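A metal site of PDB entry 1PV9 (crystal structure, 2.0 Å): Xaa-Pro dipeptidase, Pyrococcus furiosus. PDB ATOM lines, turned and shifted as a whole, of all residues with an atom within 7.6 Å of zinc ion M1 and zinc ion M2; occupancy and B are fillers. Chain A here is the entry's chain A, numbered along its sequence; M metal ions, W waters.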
ATOM      1  N   PHE A 178      10.069  19.728   9.988  1.00  0.00           N
ATOM      2  CA  PHE A 178      10.548  20.384   8.784  1.00  0.00           C
ATOM      3  C   PHE A 178      11.814  19.679   8.316  1.00  0.00           C
ATOM      4  O   PHE A 178      12.394  18.879   9.064  1.00  0.00           O
ATOM      5  CB  PHE A 178      10.819  21.887   9.034  1.00  0.00           C
ATOM      6  CG  PHE A 178      11.779  22.147  10.158  1.00  0.00           C
ATOM      7  CD1 PHE A 178      13.147  22.280   9.922  1.00  0.00           C
ATOM      8  CD2 PHE A 178      11.316  22.277  11.473  1.00  0.00           C
ATOM      9  CE1 PHE A 178      14.032  22.530  10.968  1.00  0.00           C
ATOM     10  CE2 PHE A 178      12.195  22.520  12.522  1.00  0.00           C
ATOM     11  CZ  PHE A 178      13.549  22.644  12.271  1.00  0.00           C
ATOM     12  N   ILE A 181      18.033  20.521   9.052  1.00  0.00           N
ATOM     13  CA  ILE A 181      19.200  21.276   8.634  1.00  0.00           C
ATOM     14  C   ILE A 181      20.441  20.722   9.326  1.00  0.00           C
ATOM     15  O   ILE A 181      20.555  20.757  10.550  1.00  0.00           O
ATOM     16  CB  ILE A 181      19.005  22.788   8.926  1.00  0.00           C
ATOM     17  CG1 ILE A 181      17.976  23.404   7.963  1.00  0.00           C
ATOM     18  CG2 ILE A 181      20.337  23.551   8.844  1.00  0.00           C
ATOM     19  CD1 ILE A 181      17.133  24.492   8.582  1.00  0.00           C
ATOM     20  N   PRO A 191      21.255  30.066   6.652  1.00  0.00           N
ATOM     21  CA  PRO A 191      20.262  29.777   7.710  1.00  0.00           C
ATOM     22  C   PRO A 191      19.384  28.562   7.414  1.00  0.00           C
ATOM     23  O   PRO A 191      19.099  27.785   8.328  1.00  0.00           O
ATOM     24  CB  PRO A 191      19.419  31.049   7.751  1.00  0.00           C
ATOM     25  CG  PRO A 191      20.351  32.124   7.306  1.00  0.00           C
ATOM     26  CD  PRO A 191      21.189  31.483   6.232  1.00  0.00           C
ATOM     27  N   HIS A 192      18.955  28.397   6.165  1.00  0.00           N
ATOM     28  CA  HIS A 192      18.126  27.251   5.775  1.00  0.00           C
ATOM     29  C   HIS A 192      18.917  26.213   4.974  1.00  0.00           C
ATOM     30  O   HIS A 192      18.442  25.682   3.971  1.00  0.00           O
ATOM     31  CB  HIS A 192      16.875  27.715   5.014  1.00  0.00           C
ATOM     32  CG  HIS A 192      15.847  28.386   5.884  1.00  0.00           C
ATOM     33  ND1 HIS A 192      15.794  28.206   7.246  1.00  0.00           N
ATOM     34  CD2 HIS A 192      14.840  29.232   5.577  1.00  0.00           C
ATOM     35  CE1 HIS A 192      14.806  28.915   7.750  1.00  0.00           C
ATOM     36  NE2 HIS A 192      14.204  29.553   6.755  1.00  0.00           N
ATOM     37  N   ILE A 208      22.923  22.502  13.434  1.00  0.00           N
ATOM     38  CA  ILE A 208      21.949  21.423  13.508  1.00  0.00           C
ATOM     39  C   ILE A 208      20.595  21.999  13.910  1.00  0.00           C
ATOM     40  O   ILE A 208      20.395  22.387  15.066  1.00  0.00           O
ATOM     41  CB  ILE A 208      22.389  20.320  14.516  1.00  0.00           C
ATOM     42  CG1 ILE A 208      23.793  19.803  14.174  1.00  0.00           C
ATOM     43  CG2 ILE A 208      21.392  19.167  14.524  1.00  0.00           C
ATOM     44  CD1 ILE A 208      24.652  19.530  15.395  1.00  0.00           C
ATOM     45  N   ASP A 209      19.695  22.066  12.951  1.00  0.00           N
ATOM     46  CA  ASP A 209      18.367  22.656  13.147  1.00  0.00           C
ATOM     47  C   ASP A 209      17.322  21.607  12.822  1.00  0.00           C
ATOM     48  O   ASP A 209      17.181  21.197  11.666  1.00  0.00           O
ATOM     49  CB  ASP A 209      18.199  23.891  12.254  1.00  0.00           C
ATOM     50  CG  ASP A 209      17.061  24.787  12.689  1.00  0.00           C
ATOM     51  OD1 ASP A 209      16.133  24.321  13.384  1.00  0.00           O
ATOM     52  OD2 ASP A 209      17.001  26.008  12.383  1.00  0.00           O
ATOM     53  N   LEU A 210      16.587  21.159  13.842  1.00  0.00           N
ATOM     54  CA  LEU A 210      15.592  20.104  13.661  1.00  0.00           C
ATOM     55  C   LEU A 210      14.380  20.299  14.564  1.00  0.00           C
ATOM     56  O   LEU A 210      14.407  21.081  15.512  1.00  0.00           O
ATOM     57  CB  LEU A 210      16.229  18.721  13.896  1.00  0.00           C
ATOM     58  CG  LEU A 210      16.887  18.405  15.242  1.00  0.00           C
ATOM     59  CD1 LEU A 210      15.874  17.933  16.271  1.00  0.00           C
ATOM     60  CD2 LEU A 210      17.991  17.360  15.069  1.00  0.00           C
ATOM     61  N   GLY A 211      13.307  19.582  14.242  1.00  0.00           N
ATOM     62  CA  GLY A 211      12.113  19.555  15.065  1.00  0.00           C
ATOM     63  C   GLY A 211      11.294  18.299  14.839  1.00  0.00           C
ATOM     64  O   GLY A 211      11.430  17.628  13.815  1.00  0.00           O
ATOM     65  N   SER A 219       7.851  21.046  17.469  1.00  0.00           N
ATOM     66  CA  SER A 219       8.986  21.490  18.274  1.00  0.00           C
ATOM     67  C   SER A 219      10.059  22.050  17.349  1.00  0.00           C
ATOM     68  O   SER A 219      10.037  21.799  16.146  1.00  0.00           O
ATOM     69  CB  SER A 219       9.550  20.327  19.073  1.00  0.00           C
ATOM     70  OG  SER A 219      10.109  19.352  18.219  1.00  0.00           O
ATOM     71  N   ASP A 220      11.001  22.787  17.932  1.00  0.00           N
ATOM     72  CA  ASP A 220      12.030  23.471  17.144  1.00  0.00           C
ATOM     73  C   ASP A 220      13.271  23.720  18.004  1.00  0.00           C
ATOM     74  O   ASP A 220      13.196  24.345  19.067  1.00  0.00           O
ATOM     75  CB  ASP A 220      11.473  24.796  16.619  1.00  0.00           C
ATOM     76  CG  ASP A 220      12.154  25.252  15.338  1.00  0.00           C
ATOM     77  OD1 ASP A 220      13.227  24.723  14.979  1.00  0.00           O
ATOM     78  OD2 ASP A 220      11.665  26.163  14.625  1.00  0.00           O
ATOM     79  N   ILE A 221      14.421  23.234  17.535  1.00  0.00           N
ATOM     80  CA  ILE A 221      15.688  23.394  18.259  1.00  0.00           C
ATOM     81  C   ILE A 221      16.884  23.548  17.297  1.00  0.00           C
ATOM     82  O   ILE A 221      16.944  22.893  16.266  1.00  0.00           O
ATOM     83  CB  ILE A 221      15.916  22.219  19.260  1.00  0.00           C
ATOM     84  CG1 ILE A 221      17.138  22.487  20.145  1.00  0.00           C
ATOM     85  CG2 ILE A 221      16.015  20.866  18.526  1.00  0.00           C
ATOM     86  CD1 ILE A 221      17.326  21.484  21.264  1.00  0.00           C
ATOM     87  N   THR A 222      17.813  24.442  17.656  1.00  0.00           N
ATOM     88  CA  THR A 222      19.065  24.568  16.926  1.00  0.00           C
ATOM     89  C   THR A 222      20.247  24.569  17.878  1.00  0.00           C
ATOM     90  O   THR A 222      20.252  25.269  18.889  1.00  0.00           O
ATOM     91  CB  THR A 222      19.099  25.850  16.059  1.00  0.00           C
ATOM     92  OG1 THR A 222      17.996  25.831  15.145  1.00  0.00           O
ATOM     93  CG2 THR A 222      20.311  25.843  15.126  1.00  0.00           C
ATOM     94  N   LEU A 282      14.379  37.181  15.214  1.00  0.00           N
ATOM     95  CA  LEU A 282      14.789  36.465  16.432  1.00  0.00           C
ATOM     96  C   LEU A 282      14.092  35.119  16.595  1.00  0.00           C
ATOM     97  O   LEU A 282      14.653  34.188  17.156  1.00  0.00           O
ATOM     98  CB  LEU A 282      14.537  37.321  17.676  1.00  0.00           C
ATOM     99  CG  LEU A 282      15.513  37.307  18.879  1.00  0.00           C
ATOM    100  CD1 LEU A 282      14.739  37.305  20.200  1.00  0.00           C
ATOM    101  CD2 LEU A 282      16.531  36.167  18.850  1.00  0.00           C
ATOM    102  N   GLY A 283      12.838  35.022  16.126  1.00  0.00           N
ATOM    103  CA  GLY A 283      12.079  33.798  16.272  1.00  0.00           C
ATOM    104  C   GLY A 283      10.671  33.845  15.730  1.00  0.00           C
ATOM    105  O   GLY A 283      10.292  34.781  15.026  1.00  0.00           O
ATOM    106  N   HIS A 284       9.887  32.829  16.090  1.00  0.00           N
ATOM    107  CA  HIS A 284       8.537  32.647  15.562  1.00  0.00           C
ATOM    108  C   HIS A 284       7.703  31.821  16.536  1.00  0.00           C
ATOM    109  O   HIS A 284       8.239  31.136  17.402  1.00  0.00           O
ATOM    110  CB  HIS A 284       8.583  31.924  14.213  1.00  0.00           C
ATOM    111  CG  HIS A 284       9.349  30.641  14.256  1.00  0.00           C
ATOM    112  ND1 HIS A 284       8.775  29.446  14.619  1.00  0.00           N
ATOM    113  CD2 HIS A 284      10.662  30.373  14.016  1.00  0.00           C
ATOM    114  CE1 HIS A 284       9.686  28.480  14.581  1.00  0.00           C
ATOM    115  NE2 HIS A 284      10.839  29.031  14.221  1.00  0.00           N
ATOM    116  N   GLY A 285       6.381  31.894  16.379  1.00  0.00           N
ATOM    117  CA  GLY A 285       5.473  31.065  17.144  1.00  0.00           C
ATOM    118  C   GLY A 285       5.520  29.624  16.691  1.00  0.00           C
ATOM    119  O   GLY A 285       5.901  29.334  15.550  1.00  0.00           O
ATOM    120  N   VAL A 286       5.174  28.719  17.593  1.00  0.00           N
ATOM    121  CA  VAL A 286       5.119  27.287  17.295  1.00  0.00           C
ATOM    122  C   VAL A 286       3.839  26.700  17.881  1.00  0.00           C
ATOM    123  O   VAL A 286       3.472  27.017  19.012  1.00  0.00           O
ATOM    124  CB  VAL A 286       6.336  26.497  17.860  1.00  0.00           C
ATOM    125  CG1 VAL A 286       6.401  25.109  17.252  1.00  0.00           C
ATOM    126  CG2 VAL A 286       7.630  27.240  17.612  1.00  0.00           C
ATOM    127  N   ILE A 290       4.826  24.693  12.318  1.00  0.00           N
ATOM    128  CA  ILE A 290       6.187  24.990  12.760  1.00  0.00           C
ATOM    129  C   ILE A 290       6.451  26.504  12.818  1.00  0.00           C
ATOM    130  O   ILE A 290       7.128  26.995  13.720  1.00  0.00           O
ATOM    131  CB  ILE A 290       7.249  24.227  11.903  1.00  0.00           C
ATOM    132  CG1 ILE A 290       8.666  24.423  12.447  1.00  0.00           C
ATOM    133  CG2 ILE A 290       7.187  24.656  10.427  1.00  0.00           C
ATOM    134  CD1 ILE A 290       8.907  23.819  13.819  1.00  0.00           C
ATOM    135  N   HIS A 291       5.873  27.233  11.864  1.00  0.00           N
ATOM    136  CA  HIS A 291       5.965  28.692  11.854  1.00  0.00           C
ATOM    137  C   HIS A 291       4.578  29.292  12.092  1.00  0.00           C
ATOM    138  O   HIS A 291       3.663  29.111  11.284  1.00  0.00           O
ATOM    139  CB  HIS A 291       6.565  29.203  10.541  1.00  0.00           C
ATOM    140  CG  HIS A 291       8.066  29.128  10.503  1.00  0.00           C
ATOM    141  ND1 HIS A 291       8.853  30.224  10.237  1.00  0.00           N
ATOM    142  CD2 HIS A 291       8.909  28.096  10.694  1.00  0.00           C
ATOM    143  CE1 HIS A 291      10.124  29.866  10.263  1.00  0.00           C
ATOM    144  NE2 HIS A 291      10.190  28.576  10.545  1.00  0.00           N
ATOM    145  N   ILE A 310       6.958  30.305  21.634  1.00  0.00           N
ATOM    146  CA  ILE A 310       7.801  30.946  20.631  1.00  0.00           C
ATOM    147  C   ILE A 310       9.202  30.338  20.605  1.00  0.00           C
ATOM    148  O   ILE A 310       9.594  29.626  21.539  1.00  0.00           O
ATOM    149  CB  ILE A 310       7.897  32.484  20.887  1.00  0.00           C
ATOM    150  CG1 ILE A 310       8.338  32.760  22.330  1.00  0.00           C
ATOM    151  CG2 ILE A 310       6.577  33.176  20.570  1.00  0.00           C
ATOM    152  CD1 ILE A 310       9.140  34.037  22.505  1.00  0.00           C
ATOM    153  N   THR A 311       9.955  30.635  19.548  1.00  0.00           N
ATOM    154  CA  THR A 311      11.378  30.321  19.522  1.00  0.00           C
ATOM    155  C   THR A 311      12.223  31.578  19.716  1.00  0.00           C
ATOM    156  O   THR A 311      11.800  32.690  19.411  1.00  0.00           O
ATOM    157  CB  THR A 311      11.782  29.632  18.196  1.00  0.00           C
ATOM    158  OG1 THR A 311      11.519  30.505  17.093  1.00  0.00           O
ATOM    159  CG2 THR A 311      10.928  28.406  17.925  1.00  0.00           C
ATOM    160  N   ILE A 312      13.422  31.370  20.242  1.00  0.00           N
ATOM    161  CA  ILE A 312      14.410  32.440  20.380  1.00  0.00           C
ATOM    162  C   ILE A 312      15.688  31.915  19.750  1.00  0.00           C
ATOM    163  O   ILE A 312      16.335  31.016  20.306  1.00  0.00           O
ATOM    164  CB  ILE A 312      14.586  32.841  21.869  1.00  0.00           C
ATOM    165  CG1 ILE A 312      13.322  33.567  22.376  1.00  0.00           C
ATOM    166  CG2 ILE A 312      15.799  33.751  22.045  1.00  0.00           C
ATOM    167  CD1 ILE A 312      13.103  33.490  23.880  1.00  0.00           C
ATOM    168  N   GLU A 313      16.026  32.447  18.585  1.00  0.00           N
ATOM    169  CA  GLU A 313      17.098  31.870  17.771  1.00  0.00           C
ATOM    170  C   GLU A 313      17.930  32.910  17.012  1.00  0.00           C
ATOM    171  O   GLU A 313      17.819  33.034  15.795  1.00  0.00           O
ATOM    172  CB  GLU A 313      16.531  30.837  16.792  1.00  0.00           C
ATOM    173  CG  GLU A 313      15.370  31.301  15.923  1.00  0.00           C
ATOM    174  CD  GLU A 313      14.885  30.245  14.950  1.00  0.00           C
ATOM    175  OE1 GLU A 313      15.710  29.550  14.321  1.00  0.00           O
ATOM    176  OE2 GLU A 313      13.655  30.103  14.813  1.00  0.00           O
ATOM    177  N   ARG A 325      24.018  29.438  14.958  1.00  0.00           N
ATOM    178  CA  ARG A 325      22.665  29.689  15.431  1.00  0.00           C
ATOM    179  C   ARG A 325      22.395  28.812  16.646  1.00  0.00           C
ATOM    180  O   ARG A 325      22.798  27.647  16.676  1.00  0.00           O
ATOM    181  CB  ARG A 325      21.626  29.436  14.336  1.00  0.00           C
ATOM    182  CG  ARG A 325      20.170  29.606  14.773  1.00  0.00           C
ATOM    183  CD  ARG A 325      19.155  29.709  13.625  1.00  0.00           C
ATOM    184  NE  ARG A 325      18.974  28.448  12.905  1.00  0.00           N
ATOM    185  CZ  ARG A 325      19.537  28.159  11.728  1.00  0.00           C
ATOM    186  NH1 ARG A 325      20.334  29.026  11.128  1.00  0.00           N
ATOM    187  NH2 ARG A 325      19.300  26.983  11.167  1.00  0.00           N
ATOM    188  N   GLU A 327      19.004  27.911  19.095  1.00  0.00           N
ATOM    189  CA  GLU A 327      17.556  28.077  19.175  1.00  0.00           C
ATOM    190  C   GLU A 327      16.920  27.228  20.263  1.00  0.00           C
ATOM    191  O   GLU A 327      17.239  26.042  20.402  1.00  0.00           O
ATOM    192  CB  GLU A 327      16.904  27.768  17.826  1.00  0.00           C
ATOM    193  CG  GLU A 327      15.398  27.537  17.870  1.00  0.00           C
ATOM    194  CD  GLU A 327      14.815  27.209  16.509  1.00  0.00           C
ATOM    195  OE1 GLU A 327      15.453  26.442  15.755  1.00  0.00           O
ATOM    196  OE2 GLU A 327      13.718  27.705  16.192  1.00  0.00           O
ATOM    197  N   ASP A 328      16.006  27.844  21.002  1.00  0.00           N
ATOM    198  CA  ASP A 328      15.173  27.140  21.967  1.00  0.00           C
ATOM    199  C   ASP A 328      13.691  27.313  21.649  1.00  0.00           C
ATOM    200  O   ASP A 328      13.292  28.330  21.080  1.00  0.00           O
ATOM    201  CB  ASP A 328      15.427  27.669  23.387  1.00  0.00           C
ATOM    202  CG  ASP A 328      16.627  27.037  24.031  1.00  0.00           C
ATOM    203  OD1 ASP A 328      16.737  25.790  24.020  1.00  0.00           O
ATOM    204  OD2 ASP A 328      17.519  27.709  24.599  1.00  0.00           O
ATOM    205  N   THR A 329      12.885  26.319  22.003  1.00  0.00           N
ATOM    206  CA  THR A 329      11.441  26.508  22.045  1.00  0.00           C
ATOM    207  C   THR A 329      11.084  26.959  23.465  1.00  0.00           C
ATOM    208  O   THR A 329      11.482  26.311  24.441  1.00  0.00           O
ATOM    209  CB  THR A 329      10.693  25.220  21.647  1.00  0.00           C
ATOM    210  OG1 THR A 329      10.852  25.008  20.242  1.00  0.00           O
ATOM    211  CG2 THR A 329       9.187  25.407  21.788  1.00  0.00           C
HETATM  212 ZN    ZN M   1      14.745  25.750  14.034  1.00  0.00          ZN
HETATM  213 ZN    ZN M   2      12.735  28.053  14.413  1.00  0.00          ZN
HETATM  214  O   HOH W   1      14.036  27.447  13.001  1.00  0.00           O
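Merely in contact with zinc ion M2: Thr 311 (3.8 Å).
Zinc ion M2 is bound by water W1, the side-chain carboxylate of Glu 327, a ring nitrogen (NE2) of His 284, the side-chain carboxylate of Asp 220 and the side-chain carboxylate of Glu 313. Zinc ion M2 has five donor atoms within binding distance.
The side-chain hydroxyl (OG1) of Thr 222 sits close to the side-chain carboxylate (OD2) of Asp 209 (2.9 Å). The backbone carbonyl oxygen of Asp 209 lies within hydrogen-bond range of the backbone NH of Ile 181, at 2.8 Å. The backbone NH of Glu 327 is in hydrogen-bond range of the backbone carbonyl oxygen of Thr 222 (2.9 Å). OD2 of Asp 209 lies within salt-bridge range of NH2 of Arg 325. The backbone carbonyl oxygen of His 284 sits at hydrogen-bond distance from the backbone NH of Thr 311 (2.8 Å). The backbone carbonyl oxygen of Asp 220 is in hydrogen-bond range of the side-chain hydroxyl of Thr 329. The side-chain carboxylate (OE1) of Glu 313 lies within salt-bridge range of the guanidinium group (NE) of Arg 325 (3.7 Å). OG1 of Thr 311 sits close to OE2 of Glu 313.
Residues that only touch zinc ion M1: Phe 178 (3.8 Å) and Thr 222 (3.4 Å). Of the 27 residues printed, 6 come within 4 Å of zinc ion M1.
Water W1 lies within hydrogen-bond range of the side-chain carboxylate of Glu 313 and the side-chain carboxylate of Asp 209.
Zinc ion M1 is bound by the side-chain carboxylate of Glu 327 (2.0 Å), the side-chain carboxylate of Asp 220 (2.1 Å), the side-chain carboxylate of Asp 209 (2.1 Å) and water W1 (2.1 Å). Zinc ion M1 has four donor atoms within binding distance. Slightly farther from zinc ion M1 lies the side-chain carboxylate (OD2) of Asp 209 (2.8 Å).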
